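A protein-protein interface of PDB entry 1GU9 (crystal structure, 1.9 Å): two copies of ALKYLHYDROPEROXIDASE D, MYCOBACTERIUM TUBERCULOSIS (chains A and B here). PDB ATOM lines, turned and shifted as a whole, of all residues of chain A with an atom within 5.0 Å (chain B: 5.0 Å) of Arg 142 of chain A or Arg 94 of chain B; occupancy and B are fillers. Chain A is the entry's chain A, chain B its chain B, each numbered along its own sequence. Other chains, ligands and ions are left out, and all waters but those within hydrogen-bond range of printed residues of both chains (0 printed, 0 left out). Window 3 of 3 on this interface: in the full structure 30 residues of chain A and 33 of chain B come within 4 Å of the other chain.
The guanidinium group (NH1) of Arg 148 of chain A is in salt-bridge range of the side-chain carboxylate (OD2) of Asp 97 of chain B (2.6 Å).
OE1 of Glu 92 of chain B sits at hydrogen-bond distance from NE2 of His 139 of chain A (3.3 Å).
The side-chain carboxylate (OE2) of Glu 138 of chain A lies close to the side-chain hydroxyl (OH) of Tyr 95 of chain B, at 2.3 Å.
The side-chain carboxylate (OE1) of Glu 138 of chain A is in salt-bridge range of the guanidinium group (NE) of Arg 94 of chain B (3.98 Å).
NH1 of Arg 148 of chain A is in hydrogen-bond range of O of Arg 94 of chain B.
NH2 of Arg 142 of chain A sits close to NH2 of Arg 94 of chain B (3.1 Å).
O of His 139 of chain A is in hydrogen-bond range of OG1 of Thr 143 of chain A (3.2 Å).
OE2 of Glu 92 of chain B is in salt-bridge range of NH2 of Arg 94 of chain B (3.4 Å).
NE of Arg 142 of chain A lies within salt-bridge range of OE1 of Glu 138 of chain A, 3.0 Å away.
Among the printed residues, pairs that only touch across the chains: Arg 148 of chain A with Tyr 95 of chain B (3.4 Å), Ile 151 of chain A with Tyr 95 of chain B (3.5 Å), Glu 138 of chain A with Leu 91 of chain B (3.99 Å) and His 139 of chain A with Arg 94 of chain B (3.996 Å).
Arg 142 of chain A touches just one residue of chain B: Arg 94.
Printed residues of chain A within 4 Å of Arg 94 of chain B: Glu 138, His 139, Arg 142 and Arg 148.
Of the printed residues of chain B, Ile 151 of chain A touches Tyr 95 (3.5 Å).
Of the printed residues of chain A, Asp 97 of chain B touches Arg 148.
Leu 141 of chain A touches none of the printed residues of chain B.
The nearest residue of chain B that does not touch Arg 142 of chain A is Tyr 95 of chain B (4.8 Å).
The nearest printed residue of chain A that does not touch Tyr 95 of chain B is Arg 142 of chain A (4.8 Å).
Of the 11 printed residues of chain A, 5 touch a printed residue of chain B.
Hydrophobic or aromatic side chains of chain A within 4 Å of the printed part of chain B: His 139 and Ile 151.
Of the 7 printed residues of chain B, 5 touch a printed residue of chain A.
Among the printed residues, Asp or Glu carboxylates within 4 Å of a Lys or Arg side-chain nitrogen of the other chain: Glu 138 of chain A with Arg 94 of chain B and Arg 148 of chain A with Asp 97 of chain B.
No position is printed for both chains.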
ATOM      1  N   GLU A 138      23.365  27.440   5.192  1.00  0.00           N
ATOM      2  CA  GLU A 138      22.535  26.292   5.547  1.00  0.00           C
ATOM      3  C   GLU A 138      23.168  25.057   4.917  1.00  0.00           C
ATOM      4  O   GLU A 138      23.236  24.005   5.554  1.00  0.00           O
ATOM      5  CB  GLU A 138      21.102  26.459   5.003  1.00  0.00           C
ATOM      6  CG  GLU A 138      20.055  25.468   5.565  1.00  0.00           C
ATOM      7  CD  GLU A 138      19.975  24.136   4.812  1.00  0.00           C
ATOM      8  OE1 GLU A 138      20.504  24.025   3.694  1.00  0.00           O
ATOM      9  OE2 GLU A 138      19.353  23.195   5.347  1.00  0.00           O
ATOM     10  N   HIS A 139      23.625  25.183   3.672  1.00  0.00           N
ATOM     11  CA  HIS A 139      24.244  24.040   2.990  1.00  0.00           C
ATOM     12  C   HIS A 139      25.504  23.617   3.743  1.00  0.00           C
ATOM     13  O   HIS A 139      25.767  22.433   3.943  1.00  0.00           O
ATOM     14  CB  HIS A 139      24.601  24.383   1.534  1.00  0.00           C
ATOM     15  CG  HIS A 139      23.417  24.481   0.609  1.00  0.00           C
ATOM     16  ND1 HIS A 139      23.551  24.558  -0.763  1.00  0.00           N
ATOM     17  CD2 HIS A 139      22.081  24.494   0.853  1.00  0.00           C
ATOM     18  CE1 HIS A 139      22.354  24.605  -1.325  1.00  0.00           C
ATOM     19  NE2 HIS A 139      21.444  24.565  -0.367  1.00  0.00           N
ATOM     20  N   THR A 140      26.286  24.596   4.169  1.00  0.00           N
ATOM     21  CA  THR A 140      27.513  24.317   4.903  1.00  0.00           C
ATOM     22  C   THR A 140      27.239  23.632   6.244  1.00  0.00           C
ATOM     23  O   THR A 140      27.937  22.684   6.614  1.00  0.00           O
ATOM     24  CB  THR A 140      28.330  25.627   5.090  1.00  0.00           C
ATOM     25  OG1 THR A 140      28.650  26.157   3.795  1.00  0.00           O
ATOM     26  CG2 THR A 140      29.613  25.367   5.881  1.00  0.00           C
ATOM     27  N   LEU A 141      26.226  24.096   6.969  1.00  0.00           N
ATOM     28  CA  LEU A 141      25.884  23.485   8.243  1.00  0.00           C
ATOM     29  C   LEU A 141      25.657  21.989   8.026  1.00  0.00           C
ATOM     30  O   LEU A 141      26.172  21.158   8.772  1.00  0.00           O
ATOM     31  CB  LEU A 141      24.602  24.088   8.838  1.00  0.00           C
ATOM     32  CG  LEU A 141      24.566  25.352   9.720  1.00  0.00           C
ATOM     33  CD1 LEU A 141      25.771  25.376  10.630  1.00  0.00           C
ATOM     34  CD2 LEU A 141      24.494  26.595   8.891  1.00  0.00           C
ATOM     35  N   ARG A 142      24.864  21.653   7.017  1.00  0.00           N
ATOM     36  CA  ARG A 142      24.572  20.247   6.716  1.00  0.00           C
ATOM     37  C   ARG A 142      25.827  19.458   6.360  1.00  0.00           C
ATOM     38  O   ARG A 142      25.971  18.296   6.747  1.00  0.00           O
ATOM     39  CB  ARG A 142      23.542  20.144   5.589  1.00  0.00           C
ATOM     40  CG  ARG A 142      22.117  20.443   6.075  1.00  0.00           C
ATOM     41  CD  ARG A 142      21.039  20.186   5.009  1.00  0.00           C
ATOM     42  NE  ARG A 142      21.119  21.111   3.882  1.00  0.00           N
ATOM     43  CZ  ARG A 142      21.472  20.767   2.646  1.00  0.00           C
ATOM     44  NH1 ARG A 142      21.784  19.508   2.363  1.00  0.00           N
ATOM     45  NH2 ARG A 142      21.512  21.683   1.689  1.00  0.00           N
ATOM     46  N   THR A 143      26.739  20.088   5.630  1.00  0.00           N
ATOM     47  CA  THR A 143      27.979  19.429   5.257  1.00  0.00           C
ATOM     48  C   THR A 143      28.885  19.125   6.454  1.00  0.00           C
ATOM     49  O   THR A 143      29.715  18.220   6.386  1.00  0.00           O
ATOM     50  CB  THR A 143      28.752  20.274   4.245  1.00  0.00           C
ATOM     51  OG1 THR A 143      28.008  20.330   3.020  1.00  0.00           O
ATOM     52  CG2 THR A 143      30.102  19.671   3.983  1.00  0.00           C
ATOM     53  N   VAL A 144      28.724  19.867   7.547  1.00  0.00           N
ATOM     54  CA  VAL A 144      29.563  19.647   8.732  1.00  0.00           C
ATOM     55  C   VAL A 144      28.850  18.901   9.856  1.00  0.00           C
ATOM     56  O   VAL A 144      29.262  18.960  11.012  1.00  0.00           O
ATOM     57  CB  VAL A 144      30.127  20.980   9.293  1.00  0.00           C
ATOM     58  CG1 VAL A 144      30.788  21.780   8.162  1.00  0.00           C
ATOM     59  CG2 VAL A 144      29.015  21.794   9.947  1.00  0.00           C
ATOM     60  N   GLY A 145      27.759  18.227   9.520  1.00  0.00           N
ATOM     61  CA  GLY A 145      27.060  17.440  10.513  1.00  0.00           C
ATOM     62  C   GLY A 145      25.999  18.061  11.392  1.00  0.00           C
ATOM     63  O   GLY A 145      25.563  17.415  12.346  1.00  0.00           O
ATOM     64  N   VAL A 146      25.583  19.294  11.120  1.00  0.00           N
ATOM     65  CA  VAL A 146      24.531  19.879  11.943  1.00  0.00           C
ATOM     66  C   VAL A 146      23.209  19.459  11.332  1.00  0.00           C
ATOM     67  O   VAL A 146      23.000  19.613  10.132  1.00  0.00           O
ATOM     68  CB  VAL A 146      24.589  21.418  11.979  1.00  0.00           C
ATOM     69  CG1 VAL A 146      23.540  21.941  12.938  1.00  0.00           C
ATOM     70  CG2 VAL A 146      25.963  21.872  12.411  1.00  0.00           C
ATOM     71  N   ARG A 148      19.048  19.525  10.707  1.00  0.00           N
ATOM     72  CA  ARG A 148      18.096  20.598  10.466  1.00  0.00           C
ATOM     73  C   ARG A 148      17.305  20.965  11.711  1.00  0.00           C
ATOM     74  O   ARG A 148      16.775  22.070  11.814  1.00  0.00           O
ATOM     75  CB  ARG A 148      17.151  20.227   9.309  1.00  0.00           C
ATOM     76  CG  ARG A 148      16.260  19.039   9.575  1.00  0.00           C
ATOM     77  CD  ARG A 148      15.175  18.947   8.506  1.00  0.00           C
ATOM     78  NE  ARG A 148      14.055  18.124   8.951  1.00  0.00           N
ATOM     79  CZ  ARG A 148      12.810  18.247   8.505  1.00  0.00           C
ATOM     80  NH1 ARG A 148      12.517  19.165   7.584  1.00  0.00           N
ATOM     81  NH2 ARG A 148      11.854  17.475   9.004  1.00  0.00           N
ATOM     82  N   ILE A 151      19.448  23.572  12.930  1.00  0.00           N
ATOM     83  CA  ILE A 151      19.476  24.712  12.015  1.00  0.00           C
ATOM     84  C   ILE A 151      18.180  25.479  12.185  1.00  0.00           C
ATOM     85  O   ILE A 151      18.187  26.702  12.239  1.00  0.00           O
ATOM     86  CB  ILE A 151      19.638  24.255  10.569  1.00  0.00           C
ATOM     87  CG1 ILE A 151      21.022  23.612  10.409  1.00  0.00           C
ATOM     88  CG2 ILE A 151      19.477  25.446   9.598  1.00  0.00           C
ATOM     89  CD1 ILE A 151      21.313  23.142   8.986  1.00  0.00           C
ATOM     90  N   LEU B  91      14.672  28.557   2.173  1.00  0.00           N
ATOM     91  CA  LEU B  91      15.303  27.250   2.283  1.00  0.00           C
ATOM     92  C   LEU B  91      14.801  26.034   1.499  1.00  0.00           C
ATOM     93  O   LEU B  91      14.808  24.892   1.998  1.00  0.00           O
ATOM     94  CB  LEU B  91      15.461  26.931   3.779  1.00  0.00           C
ATOM     95  CG  LEU B  91      16.204  28.056   4.527  1.00  0.00           C
ATOM     96  CD1 LEU B  91      16.253  27.752   6.031  1.00  0.00           C
ATOM     97  CD2 LEU B  91      17.622  28.193   3.972  1.00  0.00           C
ATOM     98  N   GLU B  92      14.367  26.288   0.266  1.00  0.00           N
ATOM     99  CA  GLU B  92      13.989  25.219  -0.669  1.00  0.00           C
ATOM    100  C   GLU B  92      12.981  24.162  -0.211  1.00  0.00           C
ATOM    101  O   GLU B  92      13.049  23.003  -0.635  1.00  0.00           O
ATOM    102  CB  GLU B  92      15.285  24.521  -1.127  1.00  0.00           C
ATOM    103  CG  GLU B  92      16.383  25.532  -1.503  1.00  0.00           C
ATOM    104  CD  GLU B  92      17.738  24.926  -1.859  1.00  0.00           C
ATOM    105  OE1 GLU B  92      18.728  25.682  -1.885  1.00  0.00           O
ATOM    106  OE2 GLU B  92      17.833  23.720  -2.128  1.00  0.00           O
ATOM    107  N   GLY B  93      12.039  24.575   0.627  1.00  0.00           N
ATOM    108  CA  GLY B  93      11.022  23.669   1.104  1.00  0.00           C
ATOM    109  C   GLY B  93      11.560  22.678   2.127  1.00  0.00           C
ATOM    110  O   GLY B  93      10.787  21.906   2.701  1.00  0.00           O
ATOM    111  N   ARG B  94      12.866  22.709   2.377  1.00  0.00           N
ATOM    112  CA  ARG B  94      13.489  21.771   3.330  1.00  0.00           C
ATOM    113  C   ARG B  94      12.964  21.817   4.754  1.00  0.00           C
ATOM    114  O   ARG B  94      13.164  20.863   5.500  1.00  0.00           O
ATOM    115  CB  ARG B  94      14.989  21.977   3.419  1.00  0.00           C
ATOM    116  CG  ARG B  94      15.767  21.788   2.137  1.00  0.00           C
ATOM    117  CD  ARG B  94      17.239  22.094   2.409  1.00  0.00           C
ATOM    118  NE  ARG B  94      18.048  22.125   1.198  1.00  0.00           N
ATOM    119  CZ  ARG B  94      18.580  21.054   0.624  1.00  0.00           C
ATOM    120  NH1 ARG B  94      18.389  19.852   1.154  1.00  0.00           N
ATOM    121  NH2 ARG B  94      19.313  21.186  -0.476  1.00  0.00           N
ATOM    122  N   TYR B  95      12.308  22.901   5.152  1.00  0.00           N
ATOM    123  CA  TYR B  95      11.816  22.983   6.522  1.00  0.00           C
ATOM    124  C   TYR B  95      10.312  23.131   6.629  1.00  0.00           C
ATOM    125  O   TYR B  95       9.814  23.458   7.699  1.00  0.00           O
ATOM    126  CB  TYR B  95      12.500  24.151   7.263  1.00  0.00           C
ATOM    127  CG  TYR B  95      14.016  23.997   7.313  1.00  0.00           C
ATOM    128  CD1 TYR B  95      14.791  24.169   6.170  1.00  0.00           C
ATOM    129  CD2 TYR B  95      14.653  23.562   8.480  1.00  0.00           C
ATOM    130  CE1 TYR B  95      16.160  23.909   6.166  1.00  0.00           C
ATOM    131  CE2 TYR B  95      16.027  23.292   8.486  1.00  0.00           C
ATOM    132  CZ  TYR B  95      16.775  23.463   7.329  1.00  0.00           C
ATOM    133  OH  TYR B  95      18.132  23.154   7.334  1.00  0.00           O
ATOM    134  N   ASP B  96       9.582  22.885   5.542  1.00  0.00           N
ATOM    135  CA  ASP B  96       8.120  23.068   5.582  1.00  0.00           C
ATOM    136  C   ASP B  96       7.350  22.088   6.474  1.00  0.00           C
ATOM    137  O   ASP B  96       6.208  22.351   6.837  1.00  0.00           O
ATOM    138  CB  ASP B  96       7.518  22.980   4.175  1.00  0.00           C
ATOM    139  CG  ASP B  96       7.935  24.125   3.283  1.00  0.00           C
ATOM    140  OD1 ASP B  96       8.490  25.125   3.807  1.00  0.00           O
ATOM    141  OD2 ASP B  96       7.696  24.020   2.055  1.00  0.00           O
ATOM    142  N   ASP B  97       7.957  20.955   6.798  1.00  0.00           N
ATOM    143  CA  ASP B  97       7.290  19.944   7.633  1.00  0.00           C
ATOM    144  C   ASP B  97       7.612  20.005   9.122  1.00  0.00           C
ATOM    145  O   ASP B  97       7.166  19.144   9.885  1.00  0.00           O
ATOM    146  CB  ASP B  97       7.622  18.543   7.122  1.00  0.00           C
ATOM    147  CG  ASP B  97       9.109  18.264   7.126  1.00  0.00           C
ATOM    148  OD1 ASP B  97       9.497  17.105   6.888  1.00  0.00           O
ATOM    149  OD2 ASP B  97       9.891  19.210   7.368  1.00  0.00           O
